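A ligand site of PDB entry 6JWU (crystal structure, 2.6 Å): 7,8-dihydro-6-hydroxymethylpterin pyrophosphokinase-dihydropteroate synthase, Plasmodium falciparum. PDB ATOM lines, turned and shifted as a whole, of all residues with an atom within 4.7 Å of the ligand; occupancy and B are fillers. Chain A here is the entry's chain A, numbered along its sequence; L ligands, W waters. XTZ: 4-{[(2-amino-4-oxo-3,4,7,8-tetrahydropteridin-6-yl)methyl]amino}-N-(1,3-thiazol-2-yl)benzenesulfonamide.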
ATOM      1  N   GLU A 434      15.752  23.201   6.873  1.00  0.00           N
ATOM      2  CA  GLU A 434      16.695  22.248   6.242  1.00  0.00           C
ATOM      3  C   GLU A 434      15.893  21.069   5.668  1.00  0.00           C
ATOM      4  O   GLU A 434      14.733  20.890   6.098  1.00  0.00           O
ATOM      5  CB  GLU A 434      17.756  21.759   7.239  1.00  0.00           C
ATOM      6  CG  GLU A 434      17.519  20.345   7.785  1.00  0.00           C
ATOM      7  CD  GLU A 434      16.311  20.145   8.693  1.00  0.00           C
ATOM      8  OE1 GLU A 434      15.729  21.164   9.168  1.00  0.00           O
ATOM      9  OE2 GLU A 434      15.941  18.971   8.931  1.00  0.00           O
ATOM     10  N   SER A 436      16.427  16.786   5.048  1.00  0.00           N
ATOM     11  CA  SER A 436      17.236  15.641   5.558  1.00  0.00           C
ATOM     12  C   SER A 436      16.947  14.372   4.752  1.00  0.00           C
ATOM     13  O   SER A 436      17.529  13.316   5.093  1.00  0.00           O
ATOM     14  CB  SER A 436      16.995  15.450   7.029  1.00  0.00           C
ATOM     15  OG  SER A 436      17.575  16.499   7.791  1.00  0.00           O
ATOM     16  N   ALA A 437      16.120  14.462   3.700  1.00  0.00           N
ATOM     17  CA  ALA A 437      15.791  13.348   2.777  1.00  0.00           C
ATOM     18  C   ALA A 437      17.078  12.829   2.145  1.00  0.00           C
ATOM     19  O   ALA A 437      17.994  13.616   1.894  1.00  0.00           O
ATOM     20  CB  ALA A 437      14.798  13.797   1.735  1.00  0.00           C
ATOM     21  N   PRO A 438      17.213  11.521   1.867  1.00  0.00           N
ATOM     22  CA  PRO A 438      18.412  11.011   1.207  1.00  0.00           C
ATOM     23  C   PRO A 438      18.476  11.548  -0.239  1.00  0.00           C
ATOM     24  O   PRO A 438      17.461  11.527  -0.911  1.00  0.00           O
ATOM     25  CB  PRO A 438      18.212   9.482   1.247  1.00  0.00           C
ATOM     26  CG  PRO A 438      16.705   9.345   1.210  1.00  0.00           C
ATOM     27  CD  PRO A 438      16.218  10.453   2.118  1.00  0.00           C
ATOM     28  N   ASP A 482      14.189  22.385  14.350  1.00  0.00           N
ATOM     29  CA  ASP A 482      15.035  21.343  13.757  1.00  0.00           C
ATOM     30  C   ASP A 482      16.197  22.036  13.058  1.00  0.00           C
ATOM     31  O   ASP A 482      16.087  22.339  11.859  1.00  0.00           O
ATOM     32  CB  ASP A 482      14.197  20.509  12.803  1.00  0.00           C
ATOM     33  CG  ASP A 482      14.873  19.270  12.248  1.00  0.00           C
ATOM     34  OD1 ASP A 482      16.118  19.185  12.304  1.00  0.00           O
ATOM     35  OD2 ASP A 482      14.129  18.408  11.739  1.00  0.00           O
ATOM     36  N   ASN A 502      15.947  20.914  18.477  1.00  0.00           N
ATOM     37  CA  ASN A 502      15.971  19.570  17.857  1.00  0.00           C
ATOM     38  C   ASN A 502      17.216  19.485  16.987  1.00  0.00           C
ATOM     39  O   ASN A 502      17.152  19.923  15.832  1.00  0.00           O
ATOM     40  CB  ASN A 502      14.728  19.291  17.017  1.00  0.00           C
ATOM     41  CG  ASN A 502      14.786  17.932  16.355  1.00  0.00           C
ATOM     42  OD1 ASN A 502      15.550  17.069  16.784  1.00  0.00           O
ATOM     43  ND2 ASN A 502      13.999  17.723  15.311  1.00  0.00           N
ATOM     44  N   ILE A 504      19.747  17.230  15.078  1.00  0.00           N
ATOM     45  CA  ILE A 504      19.800  15.851  14.513  1.00  0.00           C
ATOM     46  C   ILE A 504      21.254  15.365  14.486  1.00  0.00           C
ATOM     47  O   ILE A 504      21.458  14.195  14.128  1.00  0.00           O
ATOM     48  CB  ILE A 504      19.120  15.779  13.119  1.00  0.00           C
ATOM     49  CG1 ILE A 504      19.808  16.658  12.074  1.00  0.00           C
ATOM     50  CG2 ILE A 504      17.659  16.115  13.241  1.00  0.00           C
ATOM     51  CD1 ILE A 504      19.655  16.121  10.679  1.00  0.00           C
ATOM     52  N   VAL A 527      16.586  17.774  21.913  1.00  0.00           N
ATOM     53  CA  VAL A 527      16.484  16.390  21.366  1.00  0.00           C
ATOM     54  C   VAL A 527      17.836  16.030  20.767  1.00  0.00           C
ATOM     55  O   VAL A 527      18.300  16.755  19.861  1.00  0.00           O
ATOM     56  CB  VAL A 527      15.372  16.287  20.314  1.00  0.00           C
ATOM     57  CG1 VAL A 527      15.147  14.863  19.823  1.00  0.00           C
ATOM     58  CG2 VAL A 527      14.076  16.872  20.839  1.00  0.00           C
ATOM     59  N   MET A 529      19.588  13.304  18.539  1.00  0.00           N
ATOM     60  CA  MET A 529      19.304  12.210  17.579  1.00  0.00           C
ATOM     61  C   MET A 529      20.630  11.575  17.096  1.00  0.00           C
ATOM     62  O   MET A 529      21.635  12.284  16.907  1.00  0.00           O
ATOM     63  CB  MET A 529      18.525  12.762  16.380  1.00  0.00           C
ATOM     64  CG  MET A 529      17.711  11.735  15.648  1.00  0.00           C
ATOM     65  SD  MET A 529      17.206  12.359  14.041  1.00  0.00           S
ATOM     66  CE  MET A 529      18.757  12.253  13.143  1.00  0.00           C
ATOM     67  N   MET A 538      24.853   9.003   4.028  1.00  0.00           N
ATOM     68  CA  MET A 538      24.374   8.290   5.239  1.00  0.00           C
ATOM     69  C   MET A 538      23.793   6.918   4.877  1.00  0.00           C
ATOM     70  O   MET A 538      23.919   6.019   5.710  1.00  0.00           O
ATOM     71  CB  MET A 538      23.329   9.095   6.021  1.00  0.00           C
ATOM     72  CG  MET A 538      21.980   9.192   5.357  1.00  0.00           C
ATOM     73  SD  MET A 538      20.884  10.117   6.441  1.00  0.00           S
ATOM     74  CE  MET A 538      19.510  10.433   5.328  1.00  0.00           C
ATOM     75  N   ASP A 539      23.195   6.755   3.695  1.00  0.00           N
ATOM     76  CA  ASP A 539      22.655   5.449   3.228  1.00  0.00           C
ATOM     77  C   ASP A 539      23.783   4.438   3.032  1.00  0.00           C
ATOM     78  O   ASP A 539      23.483   3.214   2.995  1.00  0.00           O
ATOM     79  CB  ASP A 539      21.818   5.615   1.952  1.00  0.00           C
ATOM     80  CG  ASP A 539      20.508   6.354   2.165  1.00  0.00           C
ATOM     81  OD1 ASP A 539      20.165   6.618   3.342  1.00  0.00           O
ATOM     82  OD2 ASP A 539      19.831   6.655   1.150  1.00  0.00           O
ATOM     83  N   ASP A 575      16.631  10.189  20.708  1.00  0.00           N
ATOM     84  CA  ASP A 575      15.972   9.863  19.423  1.00  0.00           C
ATOM     85  C   ASP A 575      16.918   8.991  18.623  1.00  0.00           C
ATOM     86  O   ASP A 575      18.040   9.420  18.423  1.00  0.00           O
ATOM     87  CB  ASP A 575      15.559  11.114  18.665  1.00  0.00           C
ATOM     88  CG  ASP A 575      14.845  10.787  17.364  1.00  0.00           C
ATOM     89  OD1 ASP A 575      14.821   9.595  17.009  1.00  0.00           O
ATOM     90  OD2 ASP A 575      14.341  11.728  16.701  1.00  0.00           O
ATOM     91  N   GLY A 577      17.032   8.290  15.510  1.00  0.00           N
ATOM     92  CA  GLY A 577      17.165   8.686  14.104  1.00  0.00           C
ATOM     93  C   GLY A 577      16.835   7.549  13.132  1.00  0.00           C
ATOM     94  O   GLY A 577      17.745   7.069  12.446  1.00  0.00           O
ATOM     95  N   LEU A 578      15.560   7.143  13.059  1.00  0.00           N
ATOM     96  CA  LEU A 578      15.100   6.080  12.134  1.00  0.00           C
ATOM     97  C   LEU A 578      15.361   6.533  10.699  1.00  0.00           C
ATOM     98  O   LEU A 578      15.028   7.689  10.371  1.00  0.00           O
ATOM     99  CB  LEU A 578      13.599   5.842  12.319  1.00  0.00           C
ATOM    100  CG  LEU A 578      13.144   5.261  13.653  1.00  0.00           C
ATOM    101  CD1 LEU A 578      11.627   5.195  13.686  1.00  0.00           C
ATOM    102  CD2 LEU A 578      13.738   3.880  13.895  1.00  0.00           C
ATOM    103  N   GLY A 579      15.952   5.677   9.870  1.00  0.00           N
ATOM    104  CA  GLY A 579      16.290   5.986   8.465  1.00  0.00           C
ATOM    105  C   GLY A 579      17.532   6.867   8.283  1.00  0.00           C
ATOM    106  O   GLY A 579      17.826   7.222   7.127  1.00  0.00           O
ATOM    107  N   PHE A 580      18.231   7.230   9.360  1.00  0.00           N
ATOM    108  CA  PHE A 580      19.474   8.040   9.290  1.00  0.00           C
ATOM    109  C   PHE A 580      20.696   7.134   9.463  1.00  0.00           C
ATOM    110  O   PHE A 580      21.045   6.773  10.613  1.00  0.00           O
ATOM    111  CB  PHE A 580      19.503   9.114  10.372  1.00  0.00           C
ATOM    112  CG  PHE A 580      18.677  10.341  10.102  1.00  0.00           C
ATOM    113  CD1 PHE A 580      19.226  11.415   9.422  1.00  0.00           C
ATOM    114  CD2 PHE A 580      17.385  10.450  10.594  1.00  0.00           C
ATOM    115  CE1 PHE A 580      18.489  12.563   9.214  1.00  0.00           C
ATOM    116  CE2 PHE A 580      16.642  11.596  10.372  1.00  0.00           C
ATOM    117  CZ  PHE A 580      17.197  12.650   9.686  1.00  0.00           C
ATOM    118  N   LYS A 582      20.618   4.099   8.614  1.00  0.00           N
ATOM    119  CA  LYS A 582      20.054   2.763   8.895  1.00  0.00           C
ATOM    120  C   LYS A 582      19.345   2.206   7.643  1.00  0.00           C
ATOM    121  O   LYS A 582      18.567   2.919   7.020  1.00  0.00           O
ATOM    122  CB  LYS A 582      19.077   2.813  10.070  1.00  0.00           C
ATOM    123  CG  LYS A 582      19.712   3.106  11.424  1.00  0.00           C
ATOM    124  CD  LYS A 582      19.295   4.403  12.026  1.00  0.00           C
ATOM    125  CE  LYS A 582      20.164   4.799  13.192  1.00  0.00           C
ATOM    126  NZ  LYS A 582      20.242   6.272  13.318  1.00  0.00           N
ATOM    127  N   HIS A 584      16.415  -0.274   6.128  1.00  0.00           N
ATOM    128  CA  HIS A 584      14.998  -0.502   6.547  1.00  0.00           C
ATOM    129  C   HIS A 584      14.915  -1.566   7.638  1.00  0.00           C
ATOM    130  O   HIS A 584      14.243  -1.288   8.637  1.00  0.00           O
ATOM    131  CB  HIS A 584      14.141  -0.831   5.319  1.00  0.00           C
ATOM    132  CG  HIS A 584      14.252   0.221   4.273  1.00  0.00           C
ATOM    133  ND1 HIS A 584      14.581   1.546   4.591  1.00  0.00           N
ATOM    134  CD2 HIS A 584      14.067   0.193   2.933  1.00  0.00           C
ATOM    135  CE1 HIS A 584      14.573   2.269   3.492  1.00  0.00           C
ATOM    136  NE2 HIS A 584      14.258   1.463   2.460  1.00  0.00           N
ATOM    137  N   PHE A 603      11.909  10.278  21.993  1.00  0.00           N
ATOM    138  CA  PHE A 603      11.365  11.093  20.880  1.00  0.00           C
ATOM    139  C   PHE A 603      11.724  10.282  19.630  1.00  0.00           C
ATOM    140  O   PHE A 603      12.895   9.898  19.555  1.00  0.00           O
ATOM    141  CB  PHE A 603      11.999  12.477  20.942  1.00  0.00           C
ATOM    142  CG  PHE A 603      11.599  13.493  19.893  1.00  0.00           C
ATOM    143  CD1 PHE A 603      11.931  13.327  18.558  1.00  0.00           C
ATOM    144  CD2 PHE A 603      10.974  14.672  20.274  1.00  0.00           C
ATOM    145  CE1 PHE A 603      11.585  14.287  17.619  1.00  0.00           C
ATOM    146  CE2 PHE A 603      10.633  15.626  19.342  1.00  0.00           C
ATOM    147  CZ  PHE A 603      10.932  15.431  18.010  1.00  0.00           C
ATOM    148  N   GLY A 605      10.860   9.758  15.104  1.00  0.00           N
ATOM    149  CA  GLY A 605      10.254  10.225  13.840  1.00  0.00           C
ATOM    150  C   GLY A 605      10.202   9.109  12.821  1.00  0.00           C
ATOM    151  O   GLY A 605      11.222   8.876  12.143  1.00  0.00           O
ATOM    152  N   ARG A 608       6.383   8.997   7.407  1.00  0.00           N
ATOM    153  CA  ARG A 608       6.459   9.008   5.924  1.00  0.00           C
ATOM    154  C   ARG A 608       7.820   8.504   5.460  1.00  0.00           C
ATOM    155  O   ARG A 608       8.140   8.762   4.294  1.00  0.00           O
ATOM    156  CB  ARG A 608       6.196  10.406   5.368  1.00  0.00           C
ATOM    157  CG  ARG A 608       4.769  10.855   5.590  1.00  0.00           C
ATOM    158  CD  ARG A 608       4.527  12.202   4.956  1.00  0.00           C
ATOM    159  NE  ARG A 608       3.160  12.607   5.215  1.00  0.00           N
ATOM    160  CZ  ARG A 608       2.609  13.709   4.730  1.00  0.00           C
ATOM    161  NH1 ARG A 608       3.306  14.525   3.970  1.00  0.00           N
ATOM    162  NH2 ARG A 608       1.350  13.998   5.033  1.00  0.00           N
ATOM    163  N   LYS A 609       8.569   7.805   6.309  1.00  0.00           N
ATOM    164  CA  LYS A 609       9.933   7.354   5.951  1.00  0.00           C
ATOM    165  C   LYS A 609       9.826   6.112   5.075  1.00  0.00           C
ATOM    166  O   LYS A 609       8.804   5.413   5.161  1.00  0.00           O
ATOM    167  CB  LYS A 609      10.801   7.163   7.195  1.00  0.00           C
ATOM    168  CG  LYS A 609      11.169   8.508   7.811  1.00  0.00           C
ATOM    169  CD  LYS A 609      12.065   8.453   8.991  1.00  0.00           C
ATOM    170  CE  LYS A 609      12.485   9.855   9.345  1.00  0.00           C
ATOM    171  NZ  LYS A 609      13.038   9.965  10.707  1.00  0.00           N
ATOM    172  N   ARG A 610      10.843   5.896   4.256  1.00  0.00           N
ATOM    173  CA  ARG A 610      10.868   4.821   3.238  1.00  0.00           C
ATOM    174  C   ARG A 610      10.704   3.459   3.908  1.00  0.00           C
ATOM    175  O   ARG A 610      10.147   2.573   3.295  1.00  0.00           O
ATOM    176  CB  ARG A 610      12.147   4.943   2.406  1.00  0.00           C
ATOM    177  CG  ARG A 610      12.181   6.174   1.516  1.00  0.00           C
ATOM    178  CD  ARG A 610      13.497   6.318   0.782  1.00  0.00           C
ATOM    179  NE  ARG A 610      13.633   7.561   0.019  1.00  0.00           N
ATOM    180  CZ  ARG A 610      13.035   7.822  -1.146  1.00  0.00           C
ATOM    181  NH1 ARG A 610      12.203   6.946  -1.702  1.00  0.00           N
ATOM    182  NH2 ARG A 610      13.258   8.977  -1.760  1.00  0.00           N
ATOM    183  N   PHE A 611      11.186   3.286   5.136  1.00  0.00           N
ATOM    184  CA  PHE A 611      11.234   1.932   5.757  1.00  0.00           C
ATOM    185  C   PHE A 611       9.784   1.461   5.981  1.00  0.00           C
ATOM    186  O   PHE A 611       9.513   0.258   5.875  1.00  0.00           O
ATOM    187  CB  PHE A 611      12.086   1.942   7.030  1.00  0.00           C
ATOM    188  CG  PHE A 611      11.397   2.463   8.268  1.00  0.00           C
ATOM    189  CD1 PHE A 611      10.600   1.627   9.049  1.00  0.00           C
ATOM    190  CD2 PHE A 611      11.519   3.790   8.654  1.00  0.00           C
ATOM    191  CE1 PHE A 611       9.952   2.098  10.178  1.00  0.00           C
ATOM    192  CE2 PHE A 611      10.891   4.246   9.785  1.00  0.00           C
ATOM    193  CZ  PHE A 611      10.092   3.417  10.543  1.00  0.00           C
ATOM    194  N   ARG A 686       7.064  12.455  16.245  1.00  0.00           N
ATOM    195  CA  ARG A 686       7.170  13.528  15.236  1.00  0.00           C
ATOM    196  C   ARG A 686       6.406  13.062  14.000  1.00  0.00           C
ATOM    197  O   ARG A 686       6.883  12.147  13.328  1.00  0.00           O
ATOM    198  CB  ARG A 686       8.655  13.730  14.909  1.00  0.00           C
ATOM    199  CG  ARG A 686       9.046  15.140  14.510  1.00  0.00           C
ATOM    200  CD  ARG A 686      10.491  15.112  14.036  1.00  0.00           C
ATOM    201  NE  ARG A 686      10.710  16.178  13.082  1.00  0.00           N
ATOM    202  CZ  ARG A 686      10.733  16.040  11.752  1.00  0.00           C
ATOM    203  NH1 ARG A 686      10.932  17.102  11.001  1.00  0.00           N
ATOM    204  NH2 ARG A 686      10.566  14.852  11.177  1.00  0.00           N
HETATM  205  O3  XTZ L   1      13.617  11.245  12.860  1.00  0.00           O
HETATM  206  C16 XTZ L   1      13.806  12.473  13.042  1.00  0.00           C
HETATM  207  N2  XTZ L   1      14.035  12.891  14.286  1.00  0.00           N
HETATM  208  C3  XTZ L   1      13.812  13.480  11.937  1.00  0.00           C
HETATM  209  N4  XTZ L   1      13.609  13.175  10.626  1.00  0.00           N
HETATM  210  C4  XTZ L   1      13.646  14.108   9.667  1.00  0.00           C
HETATM  211  C15 XTZ L   1      13.896  15.545  10.023  1.00  0.00           C
HETATM  212  N8  XTZ L   1      14.106  15.813  11.438  1.00  0.00           N
HETATM  213  C2  XTZ L   1      14.073  14.874  12.373  1.00  0.00           C
HETATM  214  N3  XTZ L   1      14.301  15.191  13.672  1.00  0.00           N
HETATM  215  C1  XTZ L   1      14.276  14.193  14.598  1.00  0.00           C
HETATM  216  N1  XTZ L   1      14.477  14.475  15.906  1.00  0.00           N
HETATM  217  C5  XTZ L   1      13.435  13.802   8.190  1.00  0.00           C
HETATM  218  N5  XTZ L   1      14.619  13.130   7.624  1.00  0.00           N
HETATM  219  C6  XTZ L   1      14.542  11.984   6.850  1.00  0.00           C
HETATM  220  C14 XTZ L   1      13.374  11.720   6.132  1.00  0.00           C
HETATM  221  C13 XTZ L   1      13.240  10.532   5.451  1.00  0.00           C
HETATM  222  C9  XTZ L   1      14.233   9.559   5.481  1.00  0.00           C
HETATM  223  C8  XTZ L   1      15.397   9.782   6.230  1.00  0.00           C
HETATM  224  C7  XTZ L   1      15.548  10.985   6.910  1.00  0.00           C
HETATM  225  S1  XTZ L   1      13.930   8.207   4.694  1.00  0.00           S
HETATM  226  O1  XTZ L   1      13.797   7.124   5.638  1.00  0.00           O
HETATM  227  O2  XTZ L   1      12.641   8.368   4.065  1.00  0.00           O
HETATM  228  N6  XTZ L   1      14.972   7.777   3.529  1.00  0.00           N
HETATM  229  C10 XTZ L   1      15.877   6.742   3.567  1.00  0.00           C
HETATM  230  S2  XTZ L   1      16.747   6.226   2.162  1.00  0.00           S
HETATM  231  C12 XTZ L   1      17.531   4.971   3.070  1.00  0.00           C
HETATM  232  C11 XTZ L   1      17.096   4.976   4.388  1.00  0.00           C
HETATM  233  N7  XTZ L   1      16.163   5.970   4.654  1.00  0.00           N
HETATM  234  O   HOH W   1      19.936   6.174   6.029  1.00  0.00           O
HETATM  235  O   HOH W   2      13.562   9.125  14.733  1.00  0.00           O
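The side-chain carboxylate (OD2) of Asp 575 sits at hydrogen-bond distance from a nitrogen (N2) of the ligand (2.7 Å).
A nitrogen (N2) of the ligand sits at hydrogen-bond distance from the side-chain sulfur (SD) of Met 529 (3.2 Å).
The side-chain carboxylate (OD2) of Asp 482 sits at hydrogen-bond distance from a nitrogen (N8) of the ligand (2.6 Å).
The guanidinium group of Arg 686 sits close to a nitrogen (N8) of the ligand, 3.5 Å away.
An oxygen (O3) of the ligand is in hydrogen-bond range of the side-chain amino group (NZ) of Lys 609, 2.6 Å away.
The backbone NH of Arg 610 lies within hydrogen-bond range of an oxygen (O2) of the ligand, at 3.1 Å.
A nitrogen (N1) of the ligand is in hydrogen-bond range of the side-chain amide oxygen of Asn 502.
The backbone carbonyl oxygen (O) of Phe 580 lies within hydrogen-bond range of the side-chain amino group (NZ) of Lys 582, 2.9 Å away.
NZ of Lys 609 is in hydrogen-bond range of O of Leu 578, at 3.0 Å.
OD1 of Asp 575 is in hydrogen-bond range of N of Gly 577 (3.0 Å).
The side-chain amino group of Lys 609 is in hydrogen-bond range of the backbone carbonyl oxygen of Gly 605.
OG of Ser 436 sits at hydrogen-bond distance from OE2 of Glu 434 (3.2 Å).
The guanidinium group of Arg 686 lies within salt-bridge range of the side-chain carboxylate of Asp 482 (3.5 Å).
NZ of Lys 582 lies within hydrogen-bond range of O of Gly 577, 2.8 Å away.
OD2 of Asp 539 sits close to S2 of the ligand.
A nitrogen (N7) of the ligand sits close to the backbone carbonyl oxygen of Gly 579, at 3.2 Å.
The backbone carbonyl oxygen (O) of Gly 605 lies close to an oxygen (O3) of the ligand, 3.4 Å away.
Residues that only touch the ligand: Pro 438 (3.3 Å), Phe 580 (3.3 Å), Phe 603 (3.4 Å), Ser 436 (3.4 Å), Ile 504 (3.5 Å), Lys 582 (3.7 Å), His 584 (3.8 Å) and Val 527 (3.99 Å).
18 residues have an atom within 4 Å of the ligand: Ser 436, Pro 438, Asp 482, Asn 502, Ile 504, Val 527, Met 529, Asp 539, Asp 575, Gly 579, Phe 580, Lys 582, His 584, Phe 603, Gly 605, Lys 609, Arg 610 and Arg 686.
Water W2 lies within hydrogen-bond range of OD1 of Asp 575, N of Gly 605, O3 of the ligand and N of Leu 578.
Water W1 lies within hydrogen-bond range of the backbone carbonyl oxygen of Gly 579 (2.6 Å), the side-chain carboxylate of Asp 539 (2.7 Å) and the backbone NH of Lys 582 (3.4 Å).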
